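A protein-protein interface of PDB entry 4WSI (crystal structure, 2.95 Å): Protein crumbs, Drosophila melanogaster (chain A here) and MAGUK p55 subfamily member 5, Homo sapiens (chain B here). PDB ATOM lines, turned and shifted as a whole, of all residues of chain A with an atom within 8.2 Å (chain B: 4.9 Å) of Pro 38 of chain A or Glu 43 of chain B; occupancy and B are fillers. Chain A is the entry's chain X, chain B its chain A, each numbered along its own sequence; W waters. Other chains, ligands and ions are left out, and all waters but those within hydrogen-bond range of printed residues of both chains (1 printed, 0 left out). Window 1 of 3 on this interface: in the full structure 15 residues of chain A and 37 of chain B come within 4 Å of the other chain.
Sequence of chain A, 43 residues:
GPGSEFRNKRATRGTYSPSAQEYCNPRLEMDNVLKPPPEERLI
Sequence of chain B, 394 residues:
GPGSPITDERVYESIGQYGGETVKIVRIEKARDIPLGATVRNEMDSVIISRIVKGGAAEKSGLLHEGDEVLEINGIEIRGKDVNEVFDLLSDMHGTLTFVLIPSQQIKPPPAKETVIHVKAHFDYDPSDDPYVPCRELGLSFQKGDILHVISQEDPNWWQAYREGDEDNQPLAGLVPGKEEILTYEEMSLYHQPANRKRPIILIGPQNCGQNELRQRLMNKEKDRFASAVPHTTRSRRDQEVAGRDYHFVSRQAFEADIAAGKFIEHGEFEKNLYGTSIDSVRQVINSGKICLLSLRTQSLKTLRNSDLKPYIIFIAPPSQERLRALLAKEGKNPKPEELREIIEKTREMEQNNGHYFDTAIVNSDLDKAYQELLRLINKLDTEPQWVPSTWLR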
ATOM      1  N   VAL A  33      14.590 -22.835 -35.137  1.00  0.00           N
ATOM      2  CA  VAL A  33      15.430 -23.907 -34.611  1.00  0.00           C
ATOM      3  C   VAL A  33      16.313 -24.544 -35.687  1.00  0.00           C
ATOM      4  O   VAL A  33      17.245 -25.284 -35.375  1.00  0.00           O
ATOM      5  CB  VAL A  33      14.592 -24.991 -33.897  1.00  0.00           C
ATOM      6  CG1 VAL A  33      13.979 -24.433 -32.625  1.00  0.00           C
ATOM      7  CG2 VAL A  33      13.511 -25.532 -34.820  1.00  0.00           C
ATOM      8  N   LYS A  35      18.150 -22.742 -37.635  1.00  0.00           N
ATOM      9  CA  LYS A  35      19.350 -21.917 -37.625  1.00  0.00           C
ATOM     10  C   LYS A  35      20.388 -22.528 -36.692  1.00  0.00           C
ATOM     11  O   LYS A  35      20.030 -23.173 -35.705  1.00  0.00           O
ATOM     12  CB  LYS A  35      19.001 -20.487 -37.204  1.00  0.00           C
ATOM     13  CG  LYS A  35      18.266 -19.707 -38.285  1.00  0.00           C
ATOM     14  CD  LYS A  35      17.076 -18.942 -37.732  1.00  0.00           C
ATOM     15  CE  LYS A  35      16.251 -18.339 -38.863  1.00  0.00           C
ATOM     16  NZ  LYS A  35      15.052 -17.601 -38.372  1.00  0.00           N
ATOM     17  N   PRO A  36      21.680 -22.340 -37.012  1.00  0.00           N
ATOM     18  CA  PRO A  36      22.777 -22.925 -36.231  1.00  0.00           C
ATOM     19  C   PRO A  36      22.709 -22.551 -34.754  1.00  0.00           C
ATOM     20  O   PRO A  36      22.414 -21.401 -34.428  1.00  0.00           O
ATOM     21  CB  PRO A  36      24.031 -22.320 -36.878  1.00  0.00           C
ATOM     22  CG  PRO A  36      23.547 -21.139 -37.654  1.00  0.00           C
ATOM     23  CD  PRO A  36      22.184 -21.521 -38.126  1.00  0.00           C
ATOM     24  N   PRO A  37      22.980 -23.523 -33.868  1.00  0.00           N
ATOM     25  CA  PRO A  37      22.927 -23.337 -32.414  1.00  0.00           C
ATOM     26  C   PRO A  37      23.913 -22.273 -31.948  1.00  0.00           C
ATOM     27  O   PRO A  37      24.913 -22.037 -32.625  1.00  0.00           O
ATOM     28  CB  PRO A  37      23.333 -24.711 -31.872  1.00  0.00           C
ATOM     29  CG  PRO A  37      24.110 -25.342 -32.977  1.00  0.00           C
ATOM     30  CD  PRO A  37      23.444 -24.872 -34.232  1.00  0.00           C
ATOM     31  N   PRO A  38      23.625 -21.627 -30.806  1.00  0.00           N
ATOM     32  CA  PRO A  38      24.493 -20.589 -30.241  1.00  0.00           C
ATOM     33  C   PRO A  38      25.913 -21.102 -30.034  1.00  0.00           C
ATOM     34  O   PRO A  38      26.086 -22.242 -29.602  1.00  0.00           O
ATOM     35  CB  PRO A  38      23.840 -20.294 -28.888  1.00  0.00           C
ATOM     36  CG  PRO A  38      22.410 -20.657 -29.076  1.00  0.00           C
ATOM     37  CD  PRO A  38      22.416 -21.841 -29.991  1.00  0.00           C
ATOM     38  N   GLU A  39      26.911 -20.283 -30.352  1.00  0.00           N
ATOM     39  CA  GLU A  39      28.301 -20.684 -30.162  1.00  0.00           C
ATOM     40  C   GLU A  39      28.596 -20.825 -28.676  1.00  0.00           C
ATOM     41  O   GLU A  39      28.037 -20.105 -27.849  1.00  0.00           O
ATOM     42  CB  GLU A  39      29.269 -19.682 -30.801  1.00  0.00           C
ATOM     43  CG  GLU A  39      29.415 -18.367 -30.043  1.00  0.00           C
ATOM     44  CD  GLU A  39      30.703 -17.631 -30.377  1.00  0.00           C
ATOM     45  OE1 GLU A  39      30.863 -16.478 -29.921  1.00  0.00           O
ATOM     46  OE2 GLU A  39      31.556 -18.206 -31.087  1.00  0.00           O
ATOM     47  N   GLU A  40      29.464 -21.770 -28.339  1.00  0.00           N
ATOM     48  CA  GLU A  40      29.853 -21.969 -26.954  1.00  0.00           C
ATOM     49  C   GLU A  40      31.169 -21.262 -26.695  1.00  0.00           C
ATOM     50  O   GLU A  40      31.883 -20.891 -27.625  1.00  0.00           O
ATOM     51  CB  GLU A  40      29.988 -23.458 -26.637  1.00  0.00           C
ATOM     52  CG  GLU A  40      28.717 -24.256 -26.852  1.00  0.00           C
ATOM     53  CD  GLU A  40      28.916 -25.738 -26.604  1.00  0.00           C
ATOM     54  OE1 GLU A  40      29.963 -26.110 -26.035  1.00  0.00           O
ATOM     55  OE2 GLU A  40      28.030 -26.531 -26.980  1.00  0.00           O
ATOM     56  N   ARG A  41      31.482 -21.073 -25.421  1.00  0.00           N
ATOM     57  CA  ARG A  41      32.715 -20.414 -25.041  1.00  0.00           C
ATOM     58  C   ARG A  41      33.218 -20.994 -23.722  1.00  0.00           C
ATOM     59  O   ARG A  41      32.436 -21.245 -22.806  1.00  0.00           O
ATOM     60  CB  ARG A  41      32.492 -18.909 -24.933  1.00  0.00           C
ATOM     61  CG  ARG A  41      33.762 -18.104 -25.013  1.00  0.00           C
ATOM     62  CD  ARG A  41      34.129 -17.725 -26.434  1.00  0.00           C
ATOM     63  NE  ARG A  41      35.306 -16.861 -26.445  1.00  0.00           N
ATOM     64  CZ  ARG A  41      35.719 -16.169 -27.500  1.00  0.00           C
ATOM     65  NH1 ARG A  41      35.048 -16.232 -28.644  1.00  0.00           N
ATOM     66  NH2 ARG A  41      36.801 -15.408 -27.410  1.00  0.00           N
ATOM     67  N   ARG B  41      26.706 -21.203 -23.374  1.00  0.00           N
ATOM     68  CA  ARG B  41      26.088 -20.616 -24.551  1.00  0.00           C
ATOM     69  C   ARG B  41      25.022 -19.634 -24.102  1.00  0.00           C
ATOM     70  O   ARG B  41      24.513 -19.722 -22.984  1.00  0.00           O
ATOM     71  CB  ARG B  41      25.458 -21.697 -25.430  1.00  0.00           C
ATOM     72  CG  ARG B  41      24.196 -22.291 -24.842  1.00  0.00           C
ATOM     73  CD  ARG B  41      23.509 -23.250 -25.792  1.00  0.00           C
ATOM     74  NE  ARG B  41      22.193 -23.623 -25.284  1.00  0.00           N
ATOM     75  CZ  ARG B  41      21.966 -24.653 -24.476  1.00  0.00           C
ATOM     76  NH1 ARG B  41      22.969 -25.430 -24.089  1.00  0.00           N
ATOM     77  NH2 ARG B  41      20.734 -24.912 -24.060  1.00  0.00           N
ATOM     78  N   ASN B  42      24.694 -18.689 -24.972  1.00  0.00           N
ATOM     79  CA  ASN B  42      23.587 -17.781 -24.715  1.00  0.00           C
ATOM     80  C   ASN B  42      22.285 -18.297 -25.303  1.00  0.00           C
ATOM     81  O   ASN B  42      22.190 -18.559 -26.504  1.00  0.00           O
ATOM     82  CB  ASN B  42      23.881 -16.383 -25.261  1.00  0.00           C
ATOM     83  CG  ASN B  42      24.601 -15.509 -24.263  1.00  0.00           C
ATOM     84  OD1 ASN B  42      25.557 -14.817 -24.606  1.00  0.00           O
ATOM     85  ND2 ASN B  42      24.150 -15.539 -23.013  1.00  0.00           N
ATOM     86  N   GLU B  43      21.287 -18.457 -24.442  1.00  0.00           N
ATOM     87  CA  GLU B  43      19.928 -18.708 -24.886  1.00  0.00           C
ATOM     88  C   GLU B  43      19.106 -17.509 -24.448  1.00  0.00           C
ATOM     89  O   GLU B  43      18.764 -17.387 -23.271  1.00  0.00           O
ATOM     90  CB  GLU B  43      19.379 -19.990 -24.269  1.00  0.00           C
ATOM     91  CG  GLU B  43      18.469 -20.759 -25.201  1.00  0.00           C
ATOM     92  CD  GLU B  43      19.231 -21.421 -26.330  1.00  0.00           C
ATOM     93  OE1 GLU B  43      20.230 -22.110 -26.039  1.00  0.00           O
ATOM     94  OE2 GLU B  43      18.838 -21.247 -27.505  1.00  0.00           O
ATOM     95  N   MET B  44      18.809 -16.627 -25.402  1.00  0.00           N
ATOM     96  CA  MET B  44      18.240 -15.309 -25.118  1.00  0.00           C
ATOM     97  C   MET B  44      19.191 -14.520 -24.222  1.00  0.00           C
ATOM     98  O   MET B  44      20.388 -14.432 -24.499  1.00  0.00           O
ATOM     99  CB  MET B  44      16.857 -15.415 -24.468  1.00  0.00           C
ATOM    100  CG  MET B  44      15.880 -16.282 -25.224  1.00  0.00           C
ATOM    101  SD  MET B  44      14.661 -15.294 -26.089  1.00  0.00           S
ATOM    102  CE  MET B  44      13.809 -14.528 -24.712  1.00  0.00           C
ATOM    103  N   ASP B  45      18.657 -13.958 -23.144  1.00  0.00           N
ATOM    104  CA  ASP B  45      19.462 -13.173 -22.217  1.00  0.00           C
ATOM    105  C   ASP B  45      20.216 -14.065 -21.237  1.00  0.00           C
ATOM    106  O   ASP B  45      21.073 -13.599 -20.491  1.00  0.00           O
ATOM    107  CB  ASP B  45      18.576 -12.187 -21.451  1.00  0.00           C
ATOM    108  CG  ASP B  45      17.521 -12.884 -20.611  1.00  0.00           C
ATOM    109  OD1 ASP B  45      16.972 -13.910 -21.067  1.00  0.00           O
ATOM    110  OD2 ASP B  45      17.240 -12.405 -19.493  1.00  0.00           O
ATOM    111  N   SER B  46      19.895 -15.353 -21.246  1.00  0.00           N
ATOM    112  CA  SER B  46      20.439 -16.274 -20.257  1.00  0.00           C
ATOM    113  C   SER B  46      21.820 -16.818 -20.612  1.00  0.00           C
ATOM    114  O   SER B  46      22.186 -16.920 -21.785  1.00  0.00           O
ATOM    115  CB  SER B  46      19.472 -17.438 -20.019  1.00  0.00           C
ATOM    116  OG  SER B  46      18.345 -17.024 -19.267  1.00  0.00           O
ATOM    117  N   ILE B  48      23.831 -20.252 -20.194  1.00  0.00           N
ATOM    118  CA  ILE B  48      23.552 -21.652 -19.914  1.00  0.00           C
ATOM    119  C   ILE B  48      24.813 -22.492 -19.991  1.00  0.00           C
ATOM    120  O   ILE B  48      25.559 -22.409 -20.964  1.00  0.00           O
ATOM    121  CB  ILE B  48      22.523 -22.225 -20.911  1.00  0.00           C
ATOM    122  CG1 ILE B  48      21.279 -21.335 -20.966  1.00  0.00           C
ATOM    123  CG2 ILE B  48      22.153 -23.647 -20.535  1.00  0.00           C
ATOM    124  CD1 ILE B  48      20.590 -21.176 -19.636  1.00  0.00           C
ATOM    125  N   GLU B 269      15.905 -25.059 -29.168  1.00  0.00           N
ATOM    126  CA  GLU B 269      15.283 -24.136 -28.226  1.00  0.00           C
ATOM    127  C   GLU B 269      15.009 -22.776 -28.866  1.00  0.00           C
ATOM    128  O   GLU B 269      15.886 -22.194 -29.500  1.00  0.00           O
ATOM    129  CB  GLU B 269      16.165 -23.969 -26.987  1.00  0.00           C
ATOM    130  CG  GLU B 269      15.574 -23.076 -25.915  1.00  0.00           C
ATOM    131  CD  GLU B 269      16.298 -23.200 -24.590  1.00  0.00           C
ATOM    132  OE1 GLU B 269      17.201 -24.056 -24.482  1.00  0.00           O
ATOM    133  OE2 GLU B 269      15.968 -22.438 -23.658  1.00  0.00           O
HETATM  134  O   HOH W   1      25.841 -18.399 -27.269  1.00  0.00           O
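N of Ile 48 of chain B lies within hydrogen-bond range of O of Arg 41 of chain B (2.9 Å).
The side-chain carboxylate (OE1) of Glu 43 of chain B is in salt-bridge range of the guanidinium group (NE) of Arg 41 of chain B (2.6 Å).
The guanidinium group (NH2) of Arg 41 of chain B is in salt-bridge range of the side-chain carboxylate (OE1) of Glu 269 of chain B.
ND2 of Asn 42 of chain B is in hydrogen-bond range of O of Ser 46 of chain B (2.7 Å).
CG of Pro 38 of chain A touches O of Asn 42 of chain B, at 3.3 Å.
Pro 38 of chain A touches Glu 43 of chain B.
O of Glu 39 of chain A touches CA of Arg 41 of chain B (3.9 Å).
Of chain B, only Asn 42 and Glu 43 come within 4 Å of Pro 38 of chain A.
Of chain A, only Pro 38 (3.9 Å) comes within 4 Å of Glu 43 of chain B.
Of the printed residues of chain A, Arg 41 of chain B touches Glu 39 (3.9 Å).
Printed residues of chain B within 4 Å of Glu 39 of chain A: Arg 41 (3.9 Å).
Of the printed residues of chain A, Asn 42 of chain B touches Pro 38 (3.3 Å).
Pro 37 of chain A touches none of the printed residues of chain B.
Printed residues of chain A that touch a printed residue of chain B: Pro 38 and Glu 39.
Hydrophobic or aromatic side chains of chain A within 4 Å of the printed part of chain B: Pro 38.
Water W1 bridges the backbone NH of Asn 42 of chain B and the backbone carbonyl oxygen of Glu 39 of chain A.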
